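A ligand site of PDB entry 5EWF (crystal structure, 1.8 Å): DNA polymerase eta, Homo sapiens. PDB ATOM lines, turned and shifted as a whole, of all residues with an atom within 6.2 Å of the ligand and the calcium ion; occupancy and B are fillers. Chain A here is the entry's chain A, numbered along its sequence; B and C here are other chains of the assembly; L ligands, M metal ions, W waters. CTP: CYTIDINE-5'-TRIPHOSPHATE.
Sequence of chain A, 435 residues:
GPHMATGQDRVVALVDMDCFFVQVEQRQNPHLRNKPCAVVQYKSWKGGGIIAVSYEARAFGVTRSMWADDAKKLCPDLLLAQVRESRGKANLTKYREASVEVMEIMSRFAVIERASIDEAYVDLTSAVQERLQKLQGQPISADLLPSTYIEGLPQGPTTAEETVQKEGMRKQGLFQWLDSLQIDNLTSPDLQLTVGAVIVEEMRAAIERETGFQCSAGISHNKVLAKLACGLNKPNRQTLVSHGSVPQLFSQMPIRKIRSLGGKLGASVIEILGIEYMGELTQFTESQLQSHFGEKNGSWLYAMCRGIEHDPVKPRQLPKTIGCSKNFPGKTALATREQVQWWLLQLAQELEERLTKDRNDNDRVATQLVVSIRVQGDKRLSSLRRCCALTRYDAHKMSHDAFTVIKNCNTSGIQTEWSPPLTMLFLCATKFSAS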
ATOM      1  N   ASP A  16     -23.728 -14.433  26.413  1.00  0.00           N
ATOM      2  CA  ASP A  16     -24.462 -15.677  26.535  1.00  0.00           C
ATOM      3  C   ASP A  16     -25.541 -15.689  25.463  1.00  0.00           C
ATOM      4  O   ASP A  16     -26.439 -14.848  25.497  1.00  0.00           O
ATOM      5  CB  ASP A  16     -25.080 -15.802  27.936  1.00  0.00           C
ATOM      6  CG  ASP A  16     -25.591 -17.188  28.237  1.00  0.00           C
ATOM      7  OD1 ASP A  16     -26.006 -17.870  27.303  1.00  0.00           O
ATOM      8  OD2 ASP A  16     -25.573 -17.615  29.423  1.00  0.00           O
ATOM      9  N   MET A  17     -25.468 -16.618  24.518  1.00  0.00           N
ATOM     10  CA  MET A  17     -26.476 -16.626  23.461  1.00  0.00           C
ATOM     11  C   MET A  17     -27.846 -16.996  24.022  1.00  0.00           C
ATOM     12  O   MET A  17     -27.967 -17.890  24.850  1.00  0.00           O
ATOM     13  CB  MET A  17     -26.086 -17.599  22.356  1.00  0.00           C
ATOM     14  CG  MET A  17     -24.660 -17.433  21.847  1.00  0.00           C
ATOM     15  SD  MET A  17     -24.325 -15.805  21.185  1.00  0.00           S
ATOM     16  CE  MET A  17     -25.539 -15.756  19.874  1.00  0.00           C
ATOM     17  N   ASP A  18     -28.885 -16.293  23.558  1.00  0.00           N
ATOM     18  CA  ASP A  18     -30.239 -16.606  23.982  1.00  0.00           C
ATOM     19  C   ASP A  18     -30.729 -17.864  23.274  1.00  0.00           C
ATOM     20  O   ASP A  18     -30.495 -18.026  22.078  1.00  0.00           O
ATOM     21  CB  ASP A  18     -31.171 -15.443  23.641  1.00  0.00           C
ATOM     22  CG  ASP A  18     -30.778 -14.151  24.356  1.00  0.00           C
ATOM     23  OD1 ASP A  18     -30.379 -14.248  25.520  1.00  0.00           O
ATOM     24  OD2 ASP A  18     -30.910 -13.070  23.759  1.00  0.00           O
ATOM     25  N   CYS A  19     -31.414 -18.741  24.023  1.00  0.00           N
ATOM     26  CA  CYS A  19     -31.917 -20.056  23.563  1.00  0.00           C
ATOM     27  C   CYS A  19     -31.184 -20.539  22.317  1.00  0.00           C
ATOM     28  O   CYS A  19     -31.750 -20.619  21.219  1.00  0.00           O
ATOM     29  CB  CYS A  19     -33.432 -20.008  23.338  1.00  0.00           C
ATOM     30  SG  CYS A  19     -34.020 -18.634  22.313  1.00  0.00           S
ATOM     31  N   PHE A  20     -29.912 -20.852  22.490  1.00  0.00           N
ATOM     32  CA  PHE A  20     -28.970 -20.883  21.377  1.00  0.00           C
ATOM     33  C   PHE A  20     -29.379 -21.889  20.301  1.00  0.00           C
ATOM     34  O   PHE A  20     -29.492 -21.535  19.134  1.00  0.00           O
ATOM     35  CB  PHE A  20     -27.563 -21.187  21.877  1.00  0.00           C
ATOM     36  CG  PHE A  20     -26.540 -21.186  20.783  1.00  0.00           C
ATOM     37  CD1 PHE A  20     -26.460 -20.122  19.910  1.00  0.00           C
ATOM     38  CD2 PHE A  20     -25.681 -22.259  20.619  1.00  0.00           C
ATOM     39  CE1 PHE A  20     -25.531 -20.122  18.878  1.00  0.00           C
ATOM     40  CE2 PHE A  20     -24.729 -22.251  19.591  1.00  0.00           C
ATOM     41  CZ  PHE A  20     -24.664 -21.191  18.734  1.00  0.00           C
ATOM     42  N   PHE A  21     -29.587 -23.149  20.699  1.00  0.00           N
ATOM     43  CA  PHE A  21     -29.917 -24.191  19.703  1.00  0.00           C
ATOM     44  C   PHE A  21     -31.195 -23.830  18.972  1.00  0.00           C
ATOM     45  O   PHE A  21     -31.345 -24.108  17.772  1.00  0.00           O
ATOM     46  CB  PHE A  21     -30.066 -25.566  20.358  1.00  0.00           C
ATOM     47  CG  PHE A  21     -28.761 -26.224  20.765  1.00  0.00           C
ATOM     48  CD1 PHE A  21     -27.618 -25.496  20.948  1.00  0.00           C
ATOM     49  CD2 PHE A  21     -28.736 -27.599  20.973  1.00  0.00           C
ATOM     50  CE1 PHE A  21     -26.431 -26.123  21.336  1.00  0.00           C
ATOM     51  CE2 PHE A  21     -27.558 -28.230  21.341  1.00  0.00           C
ATOM     52  CZ  PHE A  21     -26.406 -27.479  21.549  1.00  0.00           C
ATOM     53  N   VAL A  22     -32.155 -23.232  19.684  1.00  0.00           N
ATOM     54  CA  VAL A  22     -33.387 -22.775  19.051  1.00  0.00           C
ATOM     55  C   VAL A  22     -33.090 -21.703  17.997  1.00  0.00           C
ATOM     56  O   VAL A  22     -33.603 -21.758  16.872  1.00  0.00           O
ATOM     57  CB  VAL A  22     -34.369 -22.273  20.117  1.00  0.00           C
ATOM     58  CG1 VAL A  22     -35.512 -21.483  19.464  1.00  0.00           C
ATOM     59  CG2 VAL A  22     -34.922 -23.457  20.900  1.00  0.00           C
ATOM     60  N   ILE A  51     -33.772 -30.134  24.813  1.00  0.00           N
ATOM     61  CA  ILE A  51     -32.494 -29.533  25.171  1.00  0.00           C
ATOM     62  C   ILE A  51     -32.564 -28.007  25.218  1.00  0.00           C
ATOM     63  O   ILE A  51     -31.812 -27.400  25.985  1.00  0.00           O
ATOM     64  CB  ILE A  51     -31.375 -30.014  24.233  1.00  0.00           C
ATOM     65  CG1 ILE A  51     -30.087 -29.199  24.413  1.00  0.00           C
ATOM     66  CG2 ILE A  51     -31.780 -29.924  22.788  1.00  0.00           C
ATOM     67  CD1 ILE A  51     -28.884 -29.908  23.880  1.00  0.00           C
ATOM     68  N   ALA A  52     -33.441 -27.378  24.427  1.00  0.00           N
ATOM     69  CA  ALA A  52     -33.518 -25.917  24.368  1.00  0.00           C
ATOM     70  C   ALA A  52     -34.934 -25.468  24.026  1.00  0.00           C
ATOM     71  O   ALA A  52     -35.653 -26.161  23.299  1.00  0.00           O
ATOM     72  CB  ALA A  52     -32.526 -25.351  23.340  1.00  0.00           C
ATOM     73  N   VAL A  53     -35.320 -24.287  24.514  1.00  0.00           N
ATOM     74  CA  VAL A  53     -36.715 -23.848  24.511  1.00  0.00           C
ATOM     75  C   VAL A  53     -36.806 -22.369  24.159  1.00  0.00           C
ATOM     76  O   VAL A  53     -36.168 -21.529  24.817  1.00  0.00           O
ATOM     77  CB  VAL A  53     -37.379 -24.079  25.890  1.00  0.00           C
ATOM     78  CG1 VAL A  53     -38.856 -23.762  25.852  1.00  0.00           C
ATOM     79  CG2 VAL A  53     -37.138 -25.502  26.352  1.00  0.00           C
ATOM     80  N   TYR A  55     -38.298 -18.573  23.958  1.00  0.00           N
ATOM     81  CA  TYR A  55     -38.946 -17.819  25.032  1.00  0.00           C
ATOM     82  C   TYR A  55     -40.473 -17.874  24.918  1.00  0.00           C
ATOM     83  O   TYR A  55     -41.166 -17.902  25.941  1.00  0.00           O
ATOM     84  CB  TYR A  55     -38.414 -16.377  25.055  1.00  0.00           C
ATOM     85  CG  TYR A  55     -37.064 -16.344  25.735  1.00  0.00           C
ATOM     86  CD1 TYR A  55     -35.908 -16.712  25.062  1.00  0.00           C
ATOM     87  CD2 TYR A  55     -36.942 -16.011  27.086  1.00  0.00           C
ATOM     88  CE1 TYR A  55     -34.671 -16.724  25.698  1.00  0.00           C
ATOM     89  CE2 TYR A  55     -35.714 -16.024  27.726  1.00  0.00           C
ATOM     90  CZ  TYR A  55     -34.569 -16.384  27.027  1.00  0.00           C
ATOM     91  OH  TYR A  55     -33.331 -16.387  27.666  1.00  0.00           O
ATOM     92  N   ARG A  58     -41.339 -21.073  26.646  1.00  0.00           N
ATOM     93  CA  ARG A  58     -41.096 -21.040  28.084  1.00  0.00           C
ATOM     94  C   ARG A  58     -42.284 -20.456  28.845  1.00  0.00           C
ATOM     95  O   ARG A  58     -42.511 -20.802  30.002  1.00  0.00           O
ATOM     96  CB  ARG A  58     -39.854 -20.233  28.416  1.00  0.00           C
ATOM     97  CG  ARG A  58     -38.584 -20.823  27.854  1.00  0.00           C
ATOM     98  CD  ARG A  58     -37.372 -19.949  28.174  1.00  0.00           C
ATOM     99  NE  ARG A  58     -36.236 -20.337  27.346  1.00  0.00           N
ATOM    100  CZ  ARG A  58     -34.972 -19.964  27.554  1.00  0.00           C
ATOM    101  NH1 ARG A  58     -34.663 -19.164  28.567  1.00  0.00           N
ATOM    102  NH2 ARG A  58     -34.013 -20.377  26.738  1.00  0.00           N
ATOM    103  N   ARG A  64     -36.065 -27.365  29.663  1.00  0.00           N
ATOM    104  CA  ARG A  64     -35.043 -28.339  29.333  1.00  0.00           C
ATOM    105  C   ARG A  64     -35.213 -29.582  30.194  1.00  0.00           C
ATOM    106  O   ARG A  64     -35.669 -29.508  31.336  1.00  0.00           O
ATOM    107  CB  ARG A  64     -33.659 -27.690  29.536  1.00  0.00           C
ATOM    108  CG  ARG A  64     -32.459 -28.607  29.540  1.00  0.00           C
ATOM    109  CD  ARG A  64     -31.199 -27.736  29.557  1.00  0.00           C
ATOM    110  NE  ARG A  64     -31.101 -26.956  30.790  1.00  0.00           N
ATOM    111  CZ  ARG A  64     -30.679 -25.689  30.832  1.00  0.00           C
ATOM    112  NH1 ARG A  64     -30.331 -25.095  29.694  1.00  0.00           N
ATOM    113  NH2 ARG A  64     -30.606 -25.031  31.984  1.00  0.00           N
ATOM    114  N   LEU A  92     -23.940 -32.884  17.513  1.00  0.00           N
ATOM    115  CA  LEU A  92     -24.134 -31.469  17.795  1.00  0.00           C
ATOM    116  C   LEU A  92     -23.286 -30.577  16.890  1.00  0.00           C
ATOM    117  O   LEU A  92     -23.118 -29.383  17.200  1.00  0.00           O
ATOM    118  CB  LEU A  92     -23.819 -31.188  19.263  1.00  0.00           C
ATOM    119  CG  LEU A  92     -24.628 -32.039  20.242  1.00  0.00           C
ATOM    120  CD1 LEU A  92     -24.199 -31.763  21.671  1.00  0.00           C
ATOM    121  CD2 LEU A  92     -26.106 -31.750  20.039  1.00  0.00           C
ATOM    122  N   SER A 116     -18.388 -22.176  27.355  1.00  0.00           N
ATOM    123  CA  SER A 116     -19.259 -23.296  27.008  1.00  0.00           C
ATOM    124  C   SER A 116     -19.494 -23.198  25.504  1.00  0.00           C
ATOM    125  O   SER A 116     -18.871 -22.370  24.835  1.00  0.00           O
ATOM    126  CB  SER A 116     -20.570 -23.249  27.778  1.00  0.00           C
ATOM    127  OG  SER A 116     -21.337 -22.127  27.331  1.00  0.00           O
ATOM    128  N   ILE A 117     -20.411 -24.001  24.988  1.00  0.00           N
ATOM    129  CA  ILE A 117     -20.710 -23.911  23.565  1.00  0.00           C
ATOM    130  C   ILE A 117     -21.241 -22.537  23.180  1.00  0.00           C
ATOM    131  O   ILE A 117     -21.077 -22.100  22.042  1.00  0.00           O
ATOM    132  CB  ILE A 117     -21.679 -25.036  23.135  1.00  0.00           C
ATOM    133  CG1 ILE A 117     -21.721 -25.151  21.620  1.00  0.00           C
ATOM    134  CG2 ILE A 117     -23.090 -24.799  23.722  1.00  0.00           C
ATOM    135  CD1 ILE A 117     -22.370 -26.436  21.153  1.00  0.00           C
ATOM    136  N   ASP A 118     -21.878 -21.809  24.118  1.00  0.00           N
ATOM    137  CA  ASP A 118     -22.514 -20.551  23.721  1.00  0.00           C
ATOM    138  C   ASP A 118     -22.238 -19.394  24.684  1.00  0.00           C
ATOM    139  O   ASP A 118     -22.976 -18.405  24.681  1.00  0.00           O
ATOM    140  CB  ASP A 118     -24.014 -20.736  23.547  1.00  0.00           C
ATOM    141  CG  ASP A 118     -24.754 -20.793  24.874  1.00  0.00           C
ATOM    142  OD1 ASP A 118     -24.167 -21.284  25.854  1.00  0.00           O
ATOM    143  OD2 ASP A 118     -25.913 -20.328  24.923  1.00  0.00           O
ATOM    144  N   GLU A 119     -21.191 -19.489  25.502  1.00  0.00           N
ATOM    145  CA  GLU A 119     -20.793 -18.398  26.382  1.00  0.00           C
ATOM    146  C   GLU A 119     -19.315 -18.106  26.203  1.00  0.00           C
ATOM    147  O   GLU A 119     -18.506 -19.020  25.994  1.00  0.00           O
ATOM    148  CB  GLU A 119     -21.042 -18.735  27.856  1.00  0.00           C
ATOM    149  CG  GLU A 119     -22.483 -18.881  28.253  1.00  0.00           C
ATOM    150  CD  GLU A 119     -22.620 -19.136  29.748  1.00  0.00           C
ATOM    151  OE1 GLU A 119     -21.588 -19.233  30.425  1.00  0.00           O
ATOM    152  OE2 GLU A 119     -23.760 -19.252  30.250  1.00  0.00           O
ATOM    153  N   LYS A 234     -32.570 -10.917  30.501  1.00  0.00           N
ATOM    154  CA  LYS A 234     -32.574 -11.799  29.321  1.00  0.00           C
ATOM    155  C   LYS A 234     -33.998 -11.815  28.780  1.00  0.00           C
ATOM    156  O   LYS A 234     -34.946 -11.691  29.551  1.00  0.00           O
ATOM    157  CB  LYS A 234     -32.136 -13.222  29.709  1.00  0.00           C
ATOM    158  CG  LYS A 234     -30.639 -13.540  29.637  1.00  0.00           C
ATOM    159  CD  LYS A 234     -30.412 -15.079  29.496  1.00  0.00           C
ATOM    160  CE  LYS A 234     -29.009 -15.471  28.946  1.00  0.00           C
ATOM    161  NZ  LYS A 234     -28.942 -15.727  27.434  1.00  0.00           N
ATOM    162  N   PRO A 235     -34.165 -11.965  27.455  1.00  0.00           N
ATOM    163  CA  PRO A 235     -33.143 -12.092  26.415  1.00  0.00           C
ATOM    164  C   PRO A 235     -32.843 -10.767  25.725  1.00  0.00           C
ATOM    165  O   PRO A 235     -33.562  -9.792  25.924  1.00  0.00           O
ATOM    166  CB  PRO A 235     -33.792 -13.058  25.420  1.00  0.00           C
ATOM    167  CG  PRO A 235     -35.268 -12.689  25.498  1.00  0.00           C
ATOM    168  CD  PRO A 235     -35.521 -12.248  26.931  1.00  0.00           C
ATOM    169  P    DT B   3     -35.311 -39.074  33.913  1.00  0.00           P
ATOM    170  OP1  DT B   3     -35.416 -39.827  35.170  1.00  0.00           O
ATOM    171  OP2  DT B   3     -36.416 -38.179  33.478  1.00  0.00           O
ATOM    172  O5'  DT B   3     -33.963 -38.205  33.959  1.00  0.00           O
ATOM    173  C5'  DT B   3     -33.850 -37.024  33.184  1.00  0.00           C
ATOM    174  C4'  DT B   3     -33.578 -37.369  31.737  1.00  0.00           C
ATOM    175  O4'  DT B   3     -33.440 -36.132  30.979  1.00  0.00           O
ATOM    176  C3'  DT B   3     -32.286 -38.129  31.489  1.00  0.00           C
ATOM    177  O3'  DT B   3     -32.400 -38.866  30.252  1.00  0.00           O
ATOM    178  C2'  DT B   3     -31.302 -36.986  31.354  1.00  0.00           C
ATOM    179  C1'  DT B   3     -32.109 -36.039  30.490  1.00  0.00           C
ATOM    180  N1   DT B   3     -31.674 -34.610  30.539  1.00  0.00           N
ATOM    181  C2   DT B   3     -31.589 -33.898  29.358  1.00  0.00           C
ATOM    182  O2   DT B   3     -31.847 -34.366  28.261  1.00  0.00           O
ATOM    183  N3   DT B   3     -31.181 -32.589  29.508  1.00  0.00           N
ATOM    184  C4   DT B   3     -30.864 -31.951  30.696  1.00  0.00           C
ATOM    185  O4   DT B   3     -30.503 -30.785  30.734  1.00  0.00           O
ATOM    186  C5   DT B   3     -30.982 -32.757  31.887  1.00  0.00           C
ATOM    187  C7   DT B   3     -30.673 -32.173  33.232  1.00  0.00           C
ATOM    188  C6   DT B   3     -31.376 -34.030  31.752  1.00  0.00           C
ATOM    189  P   8OG B   4     -31.282 -39.934  29.797  1.00  0.00           P
ATOM    190  OP1 8OG B   4     -31.990 -41.174  29.324  1.00  0.00           O
ATOM    191  OP2 8OG B   4     -30.216 -39.997  30.876  1.00  0.00           O
ATOM    192  O5' 8OG B   4     -30.614 -39.260  28.500  1.00  0.00           O
ATOM    193  C5' 8OG B   4     -29.727 -38.171  28.696  1.00  0.00           C
ATOM    194  C4' 8OG B   4     -29.305 -37.580  27.368  1.00  0.00           C
ATOM    195  O4' 8OG B   4     -29.291 -36.157  27.473  1.00  0.00           O
ATOM    196  C3' 8OG B   4     -27.880 -38.000  27.105  1.00  0.00           C
ATOM    197  O3' 8OG B   4     -27.750 -38.215  25.701  1.00  0.00           O
ATOM    198  C2' 8OG B   4     -27.041 -36.812  27.519  1.00  0.00           C
ATOM    199  C1' 8OG B   4     -27.973 -35.637  27.283  1.00  0.00           C
ATOM    200  N9  8OG B   4     -27.784 -34.482  28.192  1.00  0.00           N
ATOM    201  C8  8OG B   4     -27.565 -33.216  27.847  1.00  0.00           C
ATOM    202  N7  8OG B   4     -27.437 -32.327  28.829  1.00  0.00           N
ATOM    203  C5  8OG B   4     -27.591 -33.069  29.941  1.00  0.00           C
ATOM    204  C6  8OG B   4     -27.589 -32.778  31.389  1.00  0.00           C
ATOM    205  O6  8OG B   4     -27.397 -31.613  31.804  1.00  0.00           O
ATOM    206  N1  8OG B   4     -27.777 -33.800  32.243  1.00  0.00           N
ATOM    207  C2  8OG B   4     -27.991 -35.053  31.811  1.00  0.00           C
ATOM    208  N2  8OG B   4     -28.172 -36.024  32.744  1.00  0.00           N
ATOM    209  N3  8OG B   4     -28.013 -35.398  30.492  1.00  0.00           N
ATOM    210  C4  8OG B   4     -27.820 -34.471  29.529  1.00  0.00           C
ATOM    211  O8  8OG B   4     -27.468 -32.863  26.612  1.00  0.00           O
ATOM    212  P    DA B   5     -26.383 -38.802  25.111  1.00  0.00           P
ATOM    213  OP1  DA B   5     -26.614 -39.418  23.791  1.00  0.00           O
ATOM    214  OP2  DA B   5     -25.738 -39.537  26.219  1.00  0.00           O
ATOM    215  O5'  DA B   5     -25.473 -37.512  24.870  1.00  0.00           O
ATOM    216  C5'  DA B   5     -25.829 -36.589  23.861  1.00  0.00           C
ATOM    217  C4'  DA B   5     -24.809 -35.473  23.782  1.00  0.00           C
ATOM    218  O4'  DA B   5     -24.954 -34.629  24.936  1.00  0.00           O
ATOM    219  C3'  DA B   5     -23.354 -35.934  23.742  1.00  0.00           C
ATOM    220  O3'  DA B   5     -22.695 -35.219  22.720  1.00  0.00           O
ATOM    221  C2'  DA B   5     -22.816 -35.580  25.135  1.00  0.00           C
ATOM    222  C1'  DA B   5     -23.687 -34.374  25.502  1.00  0.00           C
ATOM    223  N9   DA B   5     -23.888 -34.176  26.942  1.00  0.00           N
ATOM    224  C8   DA B   5     -24.267 -35.106  27.871  1.00  0.00           C
ATOM    225  N7   DA B   5     -24.409 -34.599  29.083  1.00  0.00           N
ATOM    226  C5   DA B   5     -24.123 -33.249  28.914  1.00  0.00           C
ATOM    227  C6   DA B   5     -24.086 -32.167  29.811  1.00  0.00           C
ATOM    228  N6   DA B   5     -24.356 -32.290  31.109  1.00  0.00           N
ATOM    229  N1   DA B   5     -23.753 -30.948  29.314  1.00  0.00           N
ATOM    230  C2   DA B   5     -23.483 -30.834  28.013  1.00  0.00           C
ATOM    231  N3   DA B   5     -23.479 -31.794  27.078  1.00  0.00           N
ATOM    232  C4   DA B   5     -23.816 -32.978  27.599  1.00  0.00           C
ATOM    233  P    DT C   8     -24.381 -22.673  34.276  1.00  0.00           P
ATOM    234  OP1  DT C   8     -24.725 -21.248  34.434  1.00  0.00           O
ATOM    235  OP2  DT C   8     -25.327 -23.735  34.678  1.00  0.00           O
ATOM    236  O5'  DT C   8     -24.051 -22.956  32.743  1.00  0.00           O
ATOM    237  C5'  DT C   8     -22.965 -22.306  32.116  1.00  0.00           C
ATOM    238  C4'  DT C   8     -22.876 -22.733  30.657  1.00  0.00           C
ATOM    239  O4'  DT C   8     -22.601 -24.151  30.598  1.00  0.00           O
ATOM    240  C3'  DT C   8     -24.135 -22.506  29.845  1.00  0.00           C
ATOM    241  O3'  DT C   8     -23.796 -22.109  28.519  1.00  0.00           O
ATOM    242  C2'  DT C   8     -24.817 -23.880  29.862  1.00  0.00           C
ATOM    243  C1'  DT C   8     -23.614 -24.819  29.870  1.00  0.00           C
ATOM    244  N1   DT C   8     -23.871 -26.110  30.540  1.00  0.00           N
ATOM    245  C2   DT C   8     -23.605 -27.287  29.867  1.00  0.00           C
ATOM    246  O2   DT C   8     -23.147 -27.322  28.736  1.00  0.00           O
ATOM    247  N3   DT C   8     -23.881 -28.420  30.569  1.00  0.00           N
ATOM    248  C4   DT C   8     -24.386 -28.498  31.857  1.00  0.00           C
ATOM    249  O4   DT C   8     -24.605 -29.564  32.418  1.00  0.00           O
ATOM    250  C5   DT C   8     -24.650 -27.229  32.498  1.00  0.00           C
ATOM    251  C7   DT C   8     -25.204 -27.209  33.892  1.00  0.00           C
ATOM    252  C6   DT C   8     -24.394 -26.113  31.823  1.00  0.00           C
HETATM  253  N1  CTP L   1     -26.504 -27.523  28.285  1.00  0.00           N
HETATM  254  C2  CTP L   1     -26.597 -28.857  28.556  1.00  0.00           C
HETATM  255  N3  CTP L   1     -27.065 -29.271  29.775  1.00  0.00           N
HETATM  256  C4  CTP L   1     -27.561 -28.386  30.686  1.00  0.00           C
HETATM  257  C5  CTP L   1     -27.532 -27.013  30.398  1.00  0.00           C
HETATM  258  C6  CTP L   1     -27.027 -26.596  29.164  1.00  0.00           C
HETATM  259  O2  CTP L   1     -26.262 -29.680  27.709  1.00  0.00           O
HETATM  260  N4  CTP L   1     -28.046 -28.861  31.827  1.00  0.00           N
HETATM  261  C1' CTP L   1     -25.924 -27.115  26.994  1.00  0.00           C
HETATM  262  C2' CTP L   1     -26.978 -27.375  25.917  1.00  0.00           C
HETATM  263  O2' CTP L   1     -26.293 -27.812  24.774  1.00  0.00           O
HETATM  264  C3' CTP L   1     -27.570 -26.019  25.644  1.00  0.00           C
HETATM  265  C4' CTP L   1     -26.365 -25.119  25.872  1.00  0.00           C
HETATM  266  O4' CTP L   1     -25.675 -25.725  26.954  1.00  0.00           O
HETATM  267  O3' CTP L   1     -28.065 -25.976  24.314  1.00  0.00           O
HETATM  268  C5' CTP L   1     -26.749 -23.686  26.196  1.00  0.00           C
HETATM  269  O5' CTP L   1     -27.248 -23.709  27.509  1.00  0.00           O
HETATM  270  PA  CTP L   1     -28.015 -22.498  28.182  1.00  0.00           P
HETATM  271  O1A CTP L   1     -27.252 -21.222  27.977  1.00  0.00           O
HETATM  272  O2A CTP L   1     -28.238 -22.872  29.634  1.00  0.00           O
HETATM  273  O3A CTP L   1     -29.489 -22.447  27.557  1.00  0.00           O
HETATM  274  PB  CTP L   1     -30.048 -21.623  26.302  1.00  0.00           P
HETATM  275  O1B CTP L   1     -28.980 -20.917  25.508  1.00  0.00           O
HETATM  276  O2B CTP L   1     -30.864 -22.630  25.526  1.00  0.00           O
HETATM  277  O3B CTP L   1     -31.079 -20.634  27.035  1.00  0.00           O
HETATM  278  PG  CTP L   1     -30.786 -19.163  27.642  1.00  0.00           P
HETATM  279  O1G CTP L   1     -29.300 -18.981  27.676  1.00  0.00           O
HETATM  280  O2G CTP L   1     -31.529 -18.180  26.784  1.00  0.00           O
HETATM  281  O3G CTP L   1     -31.396 -19.269  29.012  1.00  0.00           O
HETATM  282 CA    CA M   1     -27.454 -19.482  26.419  1.00  0.00          CA
HETATM  283  O   HOH W   1     -29.165 -22.391  31.988  1.00  0.00           O
HETATM  284  O   HOH W   2     -25.954 -30.381  24.554  1.00  0.00           O
HETATM  285  O   HOH W   3     -28.801 -26.796  33.668  1.00  0.00           O
HETATM  286  O   HOH W   4     -23.709 -27.907  24.535  1.00  0.00           O
HETATM  287  O   HOH W   5     -33.390 -23.178  26.250  1.00  0.00           O
HETATM  288  O   HOH W   6     -29.549 -23.827  23.449  1.00  0.00           O
HETATM  289  O   HOH W   7     -32.156 -21.436  30.240  1.00  0.00           O
HETATM  290  O   HOH W   8     -32.970 -17.235  30.227  1.00  0.00           O
HETATM  291  O   HOH W   9     -30.689 -25.285  27.133  1.00  0.00           O
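O6 of 8OG 4 of chain B lies within hydrogen-bond range of a nitrogen (N4) of the ligand. N4 of the ligand lies within hydrogen-bond range of O4 of DT 3 of chain B (3.3 Å). The backbone NH (N) of Cys 19 lies within hydrogen-bond range of an oxygen (O2G) of the ligand, 2.8 Å away. N of Phe 20 sits close to O1B of the ligand, at 3.2 Å. The side-chain amino group (NZ) of Lys 234 is in salt-bridge range of an oxygen (O2G) of the ligand (3.6 Å). The guanidinium group (NH1) of Arg 58 lies within salt-bridge range of an oxygen (O3G) of the ligand. O2A of the ligand lies within salt-bridge range of NH1 of Arg 64, 3.1 Å away. The side-chain hydroxyl of Tyr 55 is in hydrogen-bond range of an oxygen (O2G) of the ligand (2.7 Å).
An oxygen (O2) of the ligand sits close to N1 of DA 5 of chain B (3.2 Å). N3 of DT 8 of chain C sits close to a nitrogen (N3) of the ligand. CA of Asp 18 touches O2G of the ligand, 3.5 Å away. CZ of Phe 21 touches O2' of the ligand, at 3.2 Å. Ile 51 touches the ligand. Ala 52 touches the ligand. CG2 of Ile 117 touches C4' of the ligand (3.9 Å). Of the 24 residues printed, 18 come within 4 Å of the ligand.
The side-chain carboxylate (OE2) of Glu 119 sits close to the side-chain carboxylate (OD2) of Asp 16, at 2.6 Å. The backbone carbonyl oxygen (O) of Asp 16 is in hydrogen-bond range of the side-chain amino group (NZ) of Lys 234 (3.3 Å). The side-chain amino group of Lys 234 is in salt-bridge range of the side-chain carboxylate of Asp 18 (2.8 Å). The guanidinium group (NH1) of Arg 58 sits close to the side-chain hydroxyl (OH) of Tyr 55 (3.2 Å). N of Asp 118 sits close to OG of Ser 116. NE of Arg 58 lies within hydrogen-bond range of O of Val 53. O3' of DT 8 of chain C sits at hydrogen-bond distance from OG of Ser 116.
Within 4 Å of the calcium ion: Asp 16, Met 17 and Asp 118.
Water W1 lies within hydrogen-bond range of an oxygen (O2A) of the ligand and the guanidinium group of Arg 64. Water W5 lies within hydrogen-bond range of O2B of the ligand (2.7 Å), N of Val 53 (2.8 Å) and NH2 of Arg 58 (2.9 Å). Water W6 lies within hydrogen-bond range of an oxygen (O2B) of the ligand, the backbone NH of Phe 21 and the backbone NH of Phe 20. Water W8 lies within hydrogen-bond range of OH of Tyr 55 (2.7 Å), O3G of the ligand (2.8 Å) and NH1 of Arg 58 (3.1 Å). Water W3 bridges a nitrogen (N4) of the ligand (2.9 Å) and the guanidinium group of Arg 64 (3.0 Å). Water W9 lies within hydrogen-bond range of NH1 of Arg 64 (2.6 Å), O of Ile 51 (2.7 Å) and O2B of the ligand (3.1 Å).
The calcium ion is bound by an oxygen (O1B) of the ligand (2.3 Å). O1G of the ligand is bound to the calcium ion. The calcium ion is bound by the backbone carbonyl oxygen (O) of Met 17, 2.3 Å away. The side-chain carboxylate (OD2) of Asp 118 binds the calcium ion (2.3 Å). The side-chain carboxylate (OD1) of Asp 16 binds the calcium ion (2.3 Å). O1A of the ligand is bound to the calcium ion.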
